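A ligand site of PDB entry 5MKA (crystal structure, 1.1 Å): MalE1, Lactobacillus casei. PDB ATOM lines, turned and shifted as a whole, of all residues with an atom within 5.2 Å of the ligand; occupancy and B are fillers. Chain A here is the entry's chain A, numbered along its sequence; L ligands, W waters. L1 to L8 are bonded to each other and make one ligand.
The backbone carbonyl oxygen (O) of Asn 46 sits close to an oxygen (O2) of LG3 L3, 3.4 Å away.
The side-chain amide nitrogen (NE2) of Gln 72 lies within hydrogen-bond range of an oxygen (O2) of LG6 L6, 3.1 Å away.
The backbone NH of Gly 47 is in hydrogen-bond range of an oxygen (O1) of LIG L1 (3.4 Å).
An oxygen (O1) of LG6 L6 sits at hydrogen-bond distance from the side-chain carboxylate of Asp 71 (2.6 Å).
The side-chain carboxylate (OD2) of Asp 16 is in hydrogen-bond range of an oxygen (O1) of LG2 L2 (2.6 Å).
The side-chain amide nitrogen of Asn 153 sits at hydrogen-bond distance from an oxygen (O5) of LG4 L4 (3.1 Å).
An oxygen (O5) of LG2 L2 is in hydrogen-bond range of the indole nitrogen (NE1) of Trp 225.
An oxygen (O1) of LG4 L4 sits at hydrogen-bond distance from the side-chain amide oxygen (OE1) of Gln 119, 2.7 Å away.
ND2 of Asn 46 sits at hydrogen-bond distance from O1 of LG3 L3, at 2.6 Å.
OG of Ser 44 sits at hydrogen-bond distance from N of Gly 47.
OD2 of Asp 16 lies within hydrogen-bond range of OG of Ser 48 (2.8 Å).
The side-chain amide nitrogen (NE2) of Gln 119 lies within hydrogen-bond range of the side-chain amide oxygen (OE1) of Gln 300 (2.9 Å).
The backbone carbonyl oxygen (O) of Asn 50 is in hydrogen-bond range of the side-chain hydroxyl (OG1) of Thr 53 (3.1 Å).
The side-chain carboxylate (OE1) of Glu 262 lies within hydrogen-bond range of the side-chain amide nitrogen (NE2) of Gln 119 (3.1 Å).
The indole nitrogen of Trp 225 is in hydrogen-bond range of the side-chain carboxylate of Asp 222.
The side-chain amide oxygen (OE1) of Gln 72 sits at hydrogen-bond distance from the backbone NH (N) of Lys 52.
ND2 of Asn 50 is in hydrogen-bond range of O of Asn 46, at 2.9 Å.
Thr 17 touches the ligand.
Gln 19 touches the ligand.
O of Pro 45 touches O2 of LG3 L3 (3.8 Å).
O of Ala 49 touches O3 of LG6 L6, 3.6 Å away.
Asn 50 touches the ligand.
CD of Lys 52 touches O1 of LG8 L8, 3.6 Å away.
Thr 53 touches the ligand.
Ala 69 touches the ligand.
CB of Tyr 155 touches O4 of LG6 L6 (3.6 Å).
OE1 of Glu 262 touches O1 of LG4 L4, at 3.5 Å.
Met 334 touches the ligand.
CB of Trp 344 touches O4 of LG8 L8, 3.1 Å away.
N of Asn 345 touches O5 of LG8 L8 (3.7 Å).
The nearest printed residue that does not touch the ligand is Ser 48 (4.1 Å).
Water W4 lies within hydrogen-bond range of OG1 of Thr 53 (2.6 Å), O1 of LG7 L7 (2.7 Å) and OD1 of Asn 50 (2.7 Å).
Water W5 bridges OD1 of Asn 345 (2.7 Å) and O5 of LG8 L8 (2.8 Å).
Water W2 lies within hydrogen-bond range of an oxygen (O2) of LG8 L8 and the side-chain amino group (NZ) of Lys 52.
Water W7 lies within hydrogen-bond range of O1 of LIG L1 (2.8 Å), OG1 of Thr 17 (2.8 Å) and O of Ser 44 (3.1 Å).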
ATOM      1  N   ASP A  16     -15.813   3.005 -28.797  1.00  0.00           N
ATOM      2  CA  ASP A  16     -15.516   2.428 -27.497  1.00  0.00           C
ATOM      3  C   ASP A  16     -15.724   0.905 -27.550  1.00  0.00           C
ATOM      4  O   ASP A  16     -16.559   0.391 -28.301  1.00  0.00           O
ATOM      5  CB  ASP A  16     -16.375   3.095 -26.408  1.00  0.00           C
ATOM      6  CG  ASP A  16     -15.919   4.488 -26.056  1.00  0.00           C
ATOM      7  OD1 ASP A  16     -15.213   5.151 -26.829  1.00  0.00           O
ATOM      8  OD2 ASP A  16     -16.233   4.976 -24.949  1.00  0.00           O
ATOM      9  N   THR A  17     -14.982   0.176 -26.720  1.00  0.00           N
ATOM     10  CA  THR A  17     -14.859  -1.290 -26.848  1.00  0.00           C
ATOM     11  C   THR A  17     -16.175  -2.069 -27.095  1.00  0.00           C
ATOM     12  O   THR A  17     -16.337  -2.772 -28.096  1.00  0.00           O
ATOM     13  CB  THR A  17     -14.097  -1.806 -25.627  1.00  0.00           C
ATOM     14  OG1 THR A  17     -12.833  -1.156 -25.602  1.00  0.00           O
ATOM     15  CG2 THR A  17     -13.917  -3.338 -25.677  1.00  0.00           C
ATOM     16  N   GLN A  19     -18.961  -1.136 -28.037  1.00  0.00           N
ATOM     17  CA  GLN A  19     -19.816  -0.574 -29.074  1.00  0.00           C
ATOM     18  C   GLN A  19     -19.548  -1.143 -30.462  1.00  0.00           C
ATOM     19  O   GLN A  19     -20.352  -0.919 -31.367  1.00  0.00           O
ATOM     20  CB  GLN A  19     -19.640   0.933 -29.119  1.00  0.00           C
ATOM     21  CG  GLN A  19     -19.877   1.583 -27.796  1.00  0.00           C
ATOM     22  CD  GLN A  19     -19.628   3.048 -27.848  1.00  0.00           C
ATOM     23  OE1 GLN A  19     -19.070   3.562 -28.821  1.00  0.00           O
ATOM     24  NE2 GLN A  19     -19.910   3.715 -26.775  1.00  0.00           N
ATOM     25  N   SER A  44     -11.111   1.887 -30.035  1.00  0.00           N
ATOM     26  CA  SER A  44     -10.002   2.822 -29.862  1.00  0.00           C
ATOM     27  C   SER A  44      -8.985   2.276 -28.856  1.00  0.00           C
ATOM     28  O   SER A  44      -9.304   1.434 -28.016  1.00  0.00           O
ATOM     29  CB  SER A  44     -10.496   4.170 -29.369  1.00  0.00           C
ATOM     30  OG  SER A  44     -11.183   4.004 -28.139  1.00  0.00           O
ATOM     31  N   PRO A  45      -7.766   2.834 -28.879  1.00  0.00           N
ATOM     32  CA  PRO A  45      -6.753   2.382 -27.898  1.00  0.00           C
ATOM     33  C   PRO A  45      -7.207   2.537 -26.463  1.00  0.00           C
ATOM     34  O   PRO A  45      -7.031   1.611 -25.673  1.00  0.00           O
ATOM     35  CB  PRO A  45      -5.521   3.211 -28.271  1.00  0.00           C
ATOM     36  CG  PRO A  45      -5.687   3.482 -29.720  1.00  0.00           C
ATOM     37  CD  PRO A  45      -7.161   3.696 -29.919  1.00  0.00           C
ATOM     38  N   ASN A  46      -7.789   3.684 -26.098  1.00  0.00           N
ATOM     39  CA  ASN A  46      -8.107   3.957 -24.698  1.00  0.00           C
ATOM     40  C   ASN A  46      -9.482   4.575 -24.459  1.00  0.00           C
ATOM     41  O   ASN A  46      -9.742   5.040 -23.344  1.00  0.00           O
ATOM     42  CB  ASN A  46      -7.000   4.831 -24.087  1.00  0.00           C
ATOM     43  CG  ASN A  46      -5.648   4.135 -24.105  1.00  0.00           C
ATOM     44  OD1 ASN A  46      -4.766   4.475 -24.923  1.00  0.00           O
ATOM     45  ND2 ASN A  46      -5.519   3.105 -23.311  1.00  0.00           N
ATOM     46  N   GLY A  47     -10.365   4.553 -25.435  1.00  0.00           N
ATOM     47  CA  GLY A  47     -11.726   4.995 -25.242  1.00  0.00           C
ATOM     48  C   GLY A  47     -11.937   6.479 -25.498  1.00  0.00           C
ATOM     49  O   GLY A  47     -11.006   7.278 -25.500  1.00  0.00           O
ATOM     50  N   SER A  48     -13.212   6.822 -25.691  1.00  0.00           N
ATOM     51  CA  SER A  48     -13.631   8.197 -25.965  1.00  0.00           C
ATOM     52  C   SER A  48     -13.208   9.175 -24.878  1.00  0.00           C
ATOM     53  O   SER A  48     -12.977  10.353 -25.174  1.00  0.00           O
ATOM     54  CB  SER A  48     -15.154   8.246 -26.154  1.00  0.00           C
ATOM     55  OG  SER A  48     -15.803   7.745 -25.012  1.00  0.00           O
ATOM     56  N   ALA A  49     -13.104   8.727 -23.623  1.00  0.00           N
ATOM     57  CA  ALA A  49     -12.665   9.628 -22.552  1.00  0.00           C
ATOM     58  C   ALA A  49     -11.193   9.995 -22.666  1.00  0.00           C
ATOM     59  O   ALA A  49     -10.735  10.877 -21.948  1.00  0.00           O
ATOM     60  CB  ALA A  49     -12.956   9.019 -21.180  1.00  0.00           C
ATOM     61  N   ASN A  50     -10.459   9.336 -23.578  1.00  0.00           N
ATOM     62  CA  ASN A  50      -9.034   9.561 -23.818  1.00  0.00           C
ATOM     63  C   ASN A  50      -8.757   9.878 -25.278  1.00  0.00           C
ATOM     64  O   ASN A  50      -7.608   9.747 -25.725  1.00  0.00           O
ATOM     65  CB  ASN A  50      -8.206   8.348 -23.370  1.00  0.00           C
ATOM     66  CG  ASN A  50      -8.300   8.152 -21.879  1.00  0.00           C
ATOM     67  OD1 ASN A  50      -7.895   9.017 -21.106  1.00  0.00           O
ATOM     68  ND2 ASN A  50      -8.853   7.029 -21.452  1.00  0.00           N
ATOM     69  N   LYS A  52      -8.412  12.614 -26.968  1.00  0.00           N
ATOM     70  CA  LYS A  52      -7.482  13.688 -27.302  1.00  0.00           C
ATOM     71  C   LYS A  52      -6.035  13.209 -27.266  1.00  0.00           C
ATOM     72  O   LYS A  52      -5.220  13.661 -28.083  1.00  0.00           O
ATOM     73  CB  LYS A  52      -7.683  14.890 -26.407  1.00  0.00           C
ATOM     74  CG  LYS A  52      -7.560  14.617 -24.945  1.00  0.00           C
ATOM     75  CD  LYS A  52      -7.650  15.879 -24.080  1.00  0.00           C
ATOM     76  CE  LYS A  52      -6.506  16.834 -24.361  1.00  0.00           C
ATOM     77  NZ  LYS A  52      -6.366  17.828 -23.318  1.00  0.00           N
ATOM     78  N   THR A  53      -5.701  12.298 -26.347  1.00  0.00           N
ATOM     79  CA  THR A  53      -4.340  11.762 -26.309  1.00  0.00           C
ATOM     80  C   THR A  53      -4.150  10.592 -27.256  1.00  0.00           C
ATOM     81  O   THR A  53      -3.067  10.440 -27.838  1.00  0.00           O
ATOM     82  CB  THR A  53      -3.967  11.358 -24.878  1.00  0.00           C
ATOM     83  OG1 THR A  53      -4.971  10.506 -24.346  1.00  0.00           O
ATOM     84  CG2 THR A  53      -3.794  12.570 -23.977  1.00  0.00           C
ATOM     85  N   ALA A  69     -15.675  12.816 -26.283  1.00  0.00           N
ATOM     86  CA  ALA A  69     -16.556  13.601 -25.419  1.00  0.00           C
ATOM     87  C   ALA A  69     -16.348  15.101 -25.658  1.00  0.00           C
ATOM     88  O   ALA A  69     -15.256  15.568 -25.965  1.00  0.00           O
ATOM     89  CB  ALA A  69     -16.266  13.260 -23.948  1.00  0.00           C
ATOM     90  N   ASP A  71     -16.031  17.825 -23.978  1.00  0.00           N
ATOM     91  CA  ASP A  71     -15.097  18.680 -23.256  1.00  0.00           C
ATOM     92  C   ASP A  71     -13.711  18.728 -23.888  1.00  0.00           C
ATOM     93  O   ASP A  71     -12.965  19.683 -23.632  1.00  0.00           O
ATOM     94  CB  ASP A  71     -14.928  18.217 -21.812  1.00  0.00           C
ATOM     95  CG  ASP A  71     -14.358  16.806 -21.711  1.00  0.00           C
ATOM     96  OD1 ASP A  71     -15.037  15.873 -22.216  1.00  0.00           O
ATOM     97  OD2 ASP A  71     -13.253  16.658 -21.124  1.00  0.00           O
ATOM     98  N   GLN A  72     -13.344  17.718 -24.661  1.00  0.00           N
ATOM     99  CA  GLN A  72     -12.033  17.654 -25.286  1.00  0.00           C
ATOM    100  C   GLN A  72     -11.920  18.518 -26.528  1.00  0.00           C
ATOM    101  O   GLN A  72     -10.809  18.661 -27.071  1.00  0.00           O
ATOM    102  CB  GLN A  72     -11.715  16.206 -25.622  1.00  0.00           C
ATOM    103  CG  GLN A  72     -11.582  15.324 -24.382  1.00  0.00           C
ATOM    104  CD  GLN A  72     -11.520  13.869 -24.736  1.00  0.00           C
ATOM    105  OE1 GLN A  72     -10.805  13.462 -25.657  1.00  0.00           O
ATOM    106  NE2 GLN A  72     -12.338  13.054 -24.040  1.00  0.00           N
ATOM    107  N   GLN A 119     -25.423  12.659 -22.296  1.00  0.00           N
ATOM    108  CA  GLN A 119     -24.947  11.888 -21.133  1.00  0.00           C
ATOM    109  C   GLN A 119     -25.086  12.694 -19.862  1.00  0.00           C
ATOM    110  O   GLN A 119     -24.443  13.734 -19.696  1.00  0.00           O
ATOM    111  CB  GLN A 119     -23.493  11.461 -21.325  1.00  0.00           C
ATOM    112  CG  GLN A 119     -23.301  10.539 -22.504  1.00  0.00           C
ATOM    113  CD  GLN A 119     -21.860  10.107 -22.693  1.00  0.00           C
ATOM    114  OE1 GLN A 119     -20.924  10.718 -22.145  1.00  0.00           O
ATOM    115  NE2 GLN A 119     -21.667   9.051 -23.479  1.00  0.00           N
ATOM    116  N   ASN A 153     -12.495  10.211  -9.041  1.00  0.00           N
ATOM    117  CA  ASN A 153     -12.957  10.562 -10.378  1.00  0.00           C
ATOM    118  C   ASN A 153     -13.658  11.912 -10.296  1.00  0.00           C
ATOM    119  O   ASN A 153     -14.712  12.045  -9.662  1.00  0.00           O
ATOM    120  CB  ASN A 153     -13.873   9.454 -10.898  1.00  0.00           C
ATOM    121  CG  ASN A 153     -14.369   9.746 -12.295  1.00  0.00           C
ATOM    122  OD1 ASN A 153     -14.964  10.786 -12.526  1.00  0.00           O
ATOM    123  ND2 ASN A 153     -14.123   8.839 -13.236  1.00  0.00           N
ATOM    124  N   ALA A 154     -13.035  12.927 -10.892  1.00  0.00           N
ATOM    125  CA  ALA A 154     -13.565  14.281 -10.814  1.00  0.00           C
ATOM    126  C   ALA A 154     -14.829  14.477 -11.639  1.00  0.00           C
ATOM    127  O   ALA A 154     -15.596  15.412 -11.366  1.00  0.00           O
ATOM    128  CB  ALA A 154     -12.503  15.276 -11.246  1.00  0.00           C
ATOM    129  N   TYR A 155     -15.049  13.644 -12.656  1.00  0.00           N
ATOM    130  CA  TYR A 155     -16.315  13.694 -13.372  1.00  0.00           C
ATOM    131  C   TYR A 155     -17.473  13.320 -12.464  1.00  0.00           C
ATOM    132  O   TYR A 155     -18.577  13.848 -12.616  1.00  0.00           O
ATOM    133  CB  TYR A 155     -16.219  12.785 -14.608  1.00  0.00           C
ATOM    134  CG  TYR A 155     -17.468  12.662 -15.439  1.00  0.00           C
ATOM    135  CD1 TYR A 155     -17.736  13.548 -16.467  1.00  0.00           C
ATOM    136  CD2 TYR A 155     -18.352  11.624 -15.215  1.00  0.00           C
ATOM    137  CE1 TYR A 155     -18.861  13.380 -17.276  1.00  0.00           C
ATOM    138  CE2 TYR A 155     -19.461  11.456 -16.017  1.00  0.00           C
ATOM    139  CZ  TYR A 155     -19.710  12.322 -17.060  1.00  0.00           C
ATOM    140  OH  TYR A 155     -20.818  12.146 -17.877  1.00  0.00           O
ATOM    141  N   ASP A 222     -24.038   6.378 -12.114  1.00  0.00           N
ATOM    142  CA  ASP A 222     -23.458   5.924 -13.377  1.00  0.00           C
ATOM    143  C   ASP A 222     -24.181   6.635 -14.514  1.00  0.00           C
ATOM    144  O   ASP A 222     -25.155   7.334 -14.281  1.00  0.00           O
ATOM    145  CB  ASP A 222     -23.545   4.407 -13.509  1.00  0.00           C
ATOM    146  CG  ASP A 222     -22.397   3.811 -14.338  1.00  0.00           C
ATOM    147  OD1 ASP A 222     -21.749   4.524 -15.128  1.00  0.00           O
ATOM    148  OD2 ASP A 222     -22.168   2.607 -14.192  1.00  0.00           O
ATOM    149  N   TRP A 225     -24.198   5.114 -20.827  1.00  0.00           N
ATOM    150  CA  TRP A 225     -23.364   4.100 -21.470  1.00  0.00           C
ATOM    151  C   TRP A 225     -23.545   2.749 -20.791  1.00  0.00           C
ATOM    152  O   TRP A 225     -23.265   1.715 -21.401  1.00  0.00           O
ATOM    153  CB  TRP A 225     -21.892   4.523 -21.469  1.00  0.00           C
ATOM    154  CG  TRP A 225     -21.389   4.917 -20.105  1.00  0.00           C
ATOM    155  CD1 TRP A 225     -20.925   4.109 -19.147  1.00  0.00           C
ATOM    156  CD2 TRP A 225     -21.400   6.252 -19.536  1.00  0.00           C
ATOM    157  NE1 TRP A 225     -20.605   4.828 -18.017  1.00  0.00           N
ATOM    158  CE2 TRP A 225     -20.897   6.147 -18.230  1.00  0.00           C
ATOM    159  CE3 TRP A 225     -21.751   7.507 -20.019  1.00  0.00           C
ATOM    160  CZ2 TRP A 225     -20.750   7.263 -17.408  1.00  0.00           C
ATOM    161  CZ3 TRP A 225     -21.597   8.598 -19.209  1.00  0.00           C
ATOM    162  CH2 TRP A 225     -21.121   8.476 -17.914  1.00  0.00           C
ATOM    163  N   GLU A 262     -21.741  13.195 -26.242  1.00  0.00           N
ATOM    164  CA  GLU A 262     -20.845  12.272 -26.921  1.00  0.00           C
ATOM    165  C   GLU A 262     -20.927  12.540 -28.419  1.00  0.00           C
ATOM    166  O   GLU A 262     -22.010  12.788 -28.936  1.00  0.00           O
ATOM    167  CB  GLU A 262     -21.224  10.821 -26.610  1.00  0.00           C
ATOM    168  CG  GLU A 262     -20.131   9.841 -26.966  1.00  0.00           C
ATOM    169  CD  GLU A 262     -18.921  10.020 -26.121  1.00  0.00           C
ATOM    170  OE1 GLU A 262     -19.045   9.805 -24.912  1.00  0.00           O
ATOM    171  OE2 GLU A 262     -17.869  10.412 -26.652  1.00  0.00           O
ATOM    172  N   GLN A 300     -28.047   4.348 -24.590  1.00  0.00           N
ATOM    173  CA  GLN A 300     -27.653   5.752 -24.611  1.00  0.00           C
ATOM    174  C   GLN A 300     -28.746   6.609 -25.245  1.00  0.00           C
ATOM    175  O   GLN A 300     -29.501   6.161 -26.117  1.00  0.00           O
ATOM    176  CB  GLN A 300     -26.306   5.948 -25.314  1.00  0.00           C
ATOM    177  CG  GLN A 300     -25.126   5.427 -24.515  1.00  0.00           C
ATOM    178  CD  GLN A 300     -23.877   6.295 -24.605  1.00  0.00           C
ATOM    179  OE1 GLN A 300     -23.946   7.504 -24.345  1.00  0.00           O
ATOM    180  NE2 GLN A 300     -22.755   5.704 -24.960  1.00  0.00           N
ATOM    181  N   MET A 334     -20.459  20.225 -19.635  1.00  0.00           N
ATOM    182  CA  MET A 334     -19.004  20.250 -19.485  1.00  0.00           C
ATOM    183  C   MET A 334     -18.422  21.348 -20.360  1.00  0.00           C
ATOM    184  O   MET A 334     -18.639  21.332 -21.590  1.00  0.00           O
ATOM    185  CB  MET A 334     -18.363  18.956 -19.931  1.00  0.00           C
ATOM    186  CG  MET A 334     -18.623  17.779 -18.994  1.00  0.00           C
ATOM    187  SD  MET A 334     -17.515  16.355 -19.286  1.00  0.00           S
ATOM    188  CE  MET A 334     -18.109  15.733 -20.857  1.00  0.00           C
ATOM    189  N   ALA A 341      -7.907  20.374 -19.722  1.00  0.00           N
ATOM    190  CA  ALA A 341      -6.897  19.371 -19.452  1.00  0.00           C
ATOM    191  C   ALA A 341      -6.321  19.544 -18.048  1.00  0.00           C
ATOM    192  O   ALA A 341      -6.203  18.583 -17.267  1.00  0.00           O
ATOM    193  CB  ALA A 341      -5.792  19.525 -20.497  1.00  0.00           C
ATOM    194  N   TRP A 344      -9.045  18.869 -15.205  1.00  0.00           N
ATOM    195  CA  TRP A 344      -9.333  17.492 -14.833  1.00  0.00           C
ATOM    196  C   TRP A 344      -8.208  16.925 -14.003  1.00  0.00           C
ATOM    197  O   TRP A 344      -8.429  16.225 -13.007  1.00  0.00           O
ATOM    198  CB  TRP A 344      -9.545  16.611 -16.054  1.00  0.00           C
ATOM    199  CG  TRP A 344     -10.803  16.836 -16.822  1.00  0.00           C
ATOM    200  CD1 TRP A 344     -10.905  17.235 -18.122  1.00  0.00           C
ATOM    201  CD2 TRP A 344     -12.152  16.651 -16.350  1.00  0.00           C
ATOM    202  NE1 TRP A 344     -12.220  17.299 -18.490  1.00  0.00           N
ATOM    203  CE2 TRP A 344     -13.006  16.947 -17.424  1.00  0.00           C
ATOM    204  CE3 TRP A 344     -12.707  16.264 -15.130  1.00  0.00           C
ATOM    205  CZ2 TRP A 344     -14.377  16.880 -17.323  1.00  0.00           C
ATOM    206  CZ3 TRP A 344     -14.083  16.189 -15.032  1.00  0.00           C
ATOM    207  CH2 TRP A 344     -14.908  16.506 -16.117  1.00  0.00           C
ATOM    208  N   ASN A 345      -6.965  17.215 -14.398  1.00  0.00           N
ATOM    209  CA  ASN A 345      -5.815  16.675 -13.688  1.00  0.00           C
ATOM    210  C   ASN A 345      -5.773  17.151 -12.252  1.00  0.00           C
ATOM    211  O   ASN A 345      -5.461  16.375 -11.336  1.00  0.00           O
ATOM    212  CB  ASN A 345      -4.554  17.097 -14.415  1.00  0.00           C
ATOM    213  CG  ASN A 345      -3.338  16.525 -13.784  1.00  0.00           C
ATOM    214  OD1 ASN A 345      -2.990  15.370 -14.026  1.00  0.00           O
ATOM    215  ND2 ASN A 345      -2.710  17.289 -12.908  1.00  0.00           N
HETATM  216  C1  LIG L   1     -12.329   1.038 -21.585  1.00  0.00           C
HETATM  217  C2  LIG L   1     -12.797   1.540 -22.934  1.00  0.00           C
HETATM  218  C3  LIG L   1     -13.794   2.694 -22.791  1.00  0.00           C
HETATM  219  C4  LIG L   1     -14.937   2.354 -21.815  1.00  0.00           C
HETATM  220  C5  LIG L   1     -14.344   1.876 -20.482  1.00  0.00           C
HETATM  221  C6  LIG L   1     -15.373   1.285 -19.548  1.00  0.00           C
HETATM  222  O1  LIG L   1     -11.676   1.966 -23.674  1.00  0.00           O
HETATM  223  O2  LIG L   1     -14.311   3.032 -24.083  1.00  0.00           O
HETATM  224  O3  LIG L   1     -15.666   3.609 -21.721  1.00  0.00           O
HETATM  225  O4  LIG L   1     -13.418   0.791 -20.732  1.00  0.00           O
HETATM  226  O5  LIG L   1     -14.657   0.782 -18.455  1.00  0.00           O
HETATM  227  C1  LG2 L   2     -16.953   3.539 -21.139  1.00  0.00           C
HETATM  228  C2  LG2 L   2     -17.955   4.429 -21.889  1.00  0.00           C
HETATM  229  C3  LG2 L   2     -17.605   5.905 -21.752  1.00  0.00           C
HETATM  230  C4  LG2 L   2     -17.447   6.230 -20.280  1.00  0.00           C
HETATM  231  C5  LG2 L   2     -16.408   5.326 -19.661  1.00  0.00           C
HETATM  232  C6  LG2 L   2     -16.173   5.613 -18.172  1.00  0.00           C
HETATM  233  O1  LG2 L   2     -18.041   4.047 -23.260  1.00  0.00           O
HETATM  234  O2  LG2 L   2     -18.667   6.671 -22.334  1.00  0.00           O
HETATM  235  O3  LG2 L   2     -17.034   7.624 -20.208  1.00  0.00           O
HETATM  236  O4  LG2 L   2     -16.866   3.974 -19.791  1.00  0.00           O
HETATM  237  O5  LG2 L   2     -17.417   5.518 -17.456  1.00  0.00           O
HETATM  238  C1  LG3 L   3      -7.969   2.295 -19.153  1.00  0.00           C
HETATM  239  C2  LG3 L   3      -7.766   1.818 -20.561  1.00  0.00           C
HETATM  240  C3  LG3 L   3      -9.147   2.205 -21.199  1.00  0.00           C
HETATM  241  C4  LG3 L   3     -10.252   1.630 -20.381  1.00  0.00           C
HETATM  242  C5  LG3 L   3     -10.178   2.022 -18.924  1.00  0.00           C
HETATM  243  C6  LG3 L   3     -11.262   1.424 -18.066  1.00  0.00           C
HETATM  244  O1  LG3 L   3      -6.752   2.555 -21.134  1.00  0.00           O
HETATM  245  O2  LG3 L   3      -9.221   1.759 -22.534  1.00  0.00           O
HETATM  246  O3  LG3 L   3     -11.530   2.087 -20.976  1.00  0.00           O
HETATM  247  O4  LG3 L   3      -8.884   1.642 -18.392  1.00  0.00           O
HETATM  248  O5  LG3 L   3     -11.131   1.946 -16.739  1.00  0.00           O
HETATM  249  C1  LG4 L   4     -17.866   8.455 -19.363  1.00  0.00           C
HETATM  250  C2  LG4 L   4     -18.197   9.720 -20.129  1.00  0.00           C
HETATM  251  C3  LG4 L   4     -16.961  10.608 -20.264  1.00  0.00           C
HETATM  252  C4  LG4 L   4     -16.305  10.806 -18.917  1.00  0.00           C
HETATM  253  C5  LG4 L   4     -16.030   9.488 -18.236  1.00  0.00           C
HETATM  254  C6  LG4 L   4     -15.495   9.742 -16.818  1.00  0.00           C
HETATM  255  O1  LG4 L   4     -18.678   9.365 -21.415  1.00  0.00           O
HETATM  256  O2  LG4 L   4     -17.382  11.876 -20.776  1.00  0.00           O
HETATM  257  O3  LG4 L   4     -15.046  11.479 -19.162  1.00  0.00           O
HETATM  258  O4  LG4 L   4     -17.227   8.740 -18.132  1.00  0.00           O
HETATM  259  O5  LG4 L   4     -15.079   8.496 -16.193  1.00  0.00           O
HETATM  260  C1  LG5 L   5      -5.322   6.399 -17.021  1.00  0.00           C
HETATM  261  C2  LG5 L   5      -4.589   5.334 -17.837  1.00  0.00           C
HETATM  262  C3  LG5 L   5      -5.589   4.627 -18.757  1.00  0.00           C
HETATM  263  C4  LG5 L   5      -6.740   4.087 -17.967  1.00  0.00           C
HETATM  264  C5  LG5 L   5      -7.389   5.188 -17.161  1.00  0.00           C
HETATM  265  C6  LG5 L   5      -8.513   4.687 -16.306  1.00  0.00           C
HETATM  266  O1  LG5 L   5      -3.551   5.903 -18.614  1.00  0.00           O
HETATM  267  O2  LG5 L   5      -4.922   3.603 -19.479  1.00  0.00           O
HETATM  268  O3  LG5 L   5      -7.743   3.650 -18.906  1.00  0.00           O
HETATM  269  O4  LG5 L   5      -6.415   5.822 -16.321  1.00  0.00           O
HETATM  270  O5  LG5 L   5      -7.967   3.849 -15.329  1.00  0.00           O
HETATM  271  C1  LG6 L   6     -14.960  12.855 -18.707  1.00  0.00           C
HETATM  272  C2  LG6 L   6     -14.376  13.679 -19.825  1.00  0.00           C
HETATM  273  C3  LG6 L   6     -12.929  13.339 -20.113  1.00  0.00           C
HETATM  274  C4  LG6 L   6     -12.150  13.478 -18.829  1.00  0.00           C
HETATM  275  C5  LG6 L   6     -12.766  12.547 -17.769  1.00  0.00           C
HETATM  276  C6  LG6 L   6     -12.069  12.701 -16.443  1.00  0.00           C
HETATM  277  O1  LG6 L   6     -15.195  13.532 -20.988  1.00  0.00           O
HETATM  278  O2  LG6 L   6     -12.397  14.142 -21.169  1.00  0.00           O
HETATM  279  O3  LG6 L   6     -10.797  13.095 -19.140  1.00  0.00           O
HETATM  280  O4  LG6 L   6     -14.131  12.916 -17.562  1.00  0.00           O
HETATM  281  O5  LG6 L   6     -12.381  11.623 -15.584  1.00  0.00           O
HETATM  282  C1  LG7 L   7      -5.356  11.516 -18.269  1.00  0.00           C
HETATM  283  C2  LG7 L   7      -4.433  10.631 -19.075  1.00  0.00           C
HETATM  284  C3  LG7 L   7      -4.948   9.189 -19.137  1.00  0.00           C
HETATM  285  C4  LG7 L   7      -5.168   8.705 -17.766  1.00  0.00           C
HETATM  286  C5  LG7 L   7      -6.073   9.609 -16.991  1.00  0.00           C
HETATM  287  C6  LG7 L   7      -6.234   9.189 -15.542  1.00  0.00           C
HETATM  288  O1  LG7 L   7      -4.194  11.245 -20.339  1.00  0.00           O
HETATM  289  O2  LG7 L   7      -4.040   8.350 -19.896  1.00  0.00           O
HETATM  290  O3  LG7 L   7      -5.833   7.392 -17.885  1.00  0.00           O
HETATM  291  O4  LG7 L   7      -5.527  10.929 -16.946  1.00  0.00           O
HETATM  292  O5  LG7 L   7      -4.934   8.990 -14.978  1.00  0.00           O
HETATM  293  C1  LG8 L   8      -9.887  14.166 -18.984  1.00  0.00           C
HETATM  294  C2  LG8 L   8      -8.921  14.300 -20.188  1.00  0.00           C
HETATM  295  C3  LG8 L   8      -7.979  13.082 -20.184  1.00  0.00           C
HETATM  296  C4  LG8 L   8      -7.321  12.888 -18.849  1.00  0.00           C
HETATM  297  C5  LG8 L   8      -8.350  12.828 -17.742  1.00  0.00           C
HETATM  298  C6  LG8 L   8      -7.738  12.777 -16.343  1.00  0.00           C
HETATM  299  O1  LG8 L   8      -9.626  14.422 -21.404  1.00  0.00           O
HETATM  300  O2  LG8 L   8      -7.008  13.351 -21.218  1.00  0.00           O
HETATM  301  O3  LG8 L   8      -6.621  11.587 -18.932  1.00  0.00           O
HETATM  302  O4  LG8 L   8      -9.139  14.014 -17.750  1.00  0.00           O
HETATM  303  O5  LG8 L   8      -6.900  13.929 -16.142  1.00  0.00           O
HETATM  304  O   HOH W   1     -12.978   3.820 -16.742  1.00  0.00           O
HETATM  305  O   HOH W   2      -5.738  15.805 -21.058  1.00  0.00           O
HETATM  306  O   HOH W   3      -4.904   7.052 -22.175  1.00  0.00           O
HETATM  307  O   HOH W   4      -6.226  10.909 -22.055  1.00  0.00           O
HETATM  308  O   HOH W   5      -4.254  13.526 -15.449  1.00  0.00           O
HETATM  309  O   HOH W   6      -8.868   1.365 -15.262  1.00  0.00           O
HETATM  310  O   HOH W   7     -11.933   1.424 -26.384  1.00  0.00           O
HETATM  311  O   HOH W   8      -1.715   9.614 -20.929  1.00  0.00           O
HETATM  312  O   HOH W   9      -2.800  13.515 -20.217  1.00  0.00           O
HETATM  313  O   HOH W  10      -7.396  -0.103 -16.790  1.00  0.00           O
HETATM  314  O   HOH W  11     -19.204   1.666 -23.782  1.00  0.00           O
HETATM  315  O   HOH W  12     -13.435  -1.673 -19.159  1.00  0.00           O
HETATM  316  O   HOH W  13     -10.873   9.603 -16.807  1.00  0.00           O
HETATM  317  O   HOH W  14     -16.807   6.796 -15.154  1.00  0.00           O
HETATM  318  O   HOH W  15     -12.826   7.464 -17.145  1.00  0.00           O
HETATM  319  O   HOH W  16      -3.489  11.224 -14.696  1.00  0.00           O
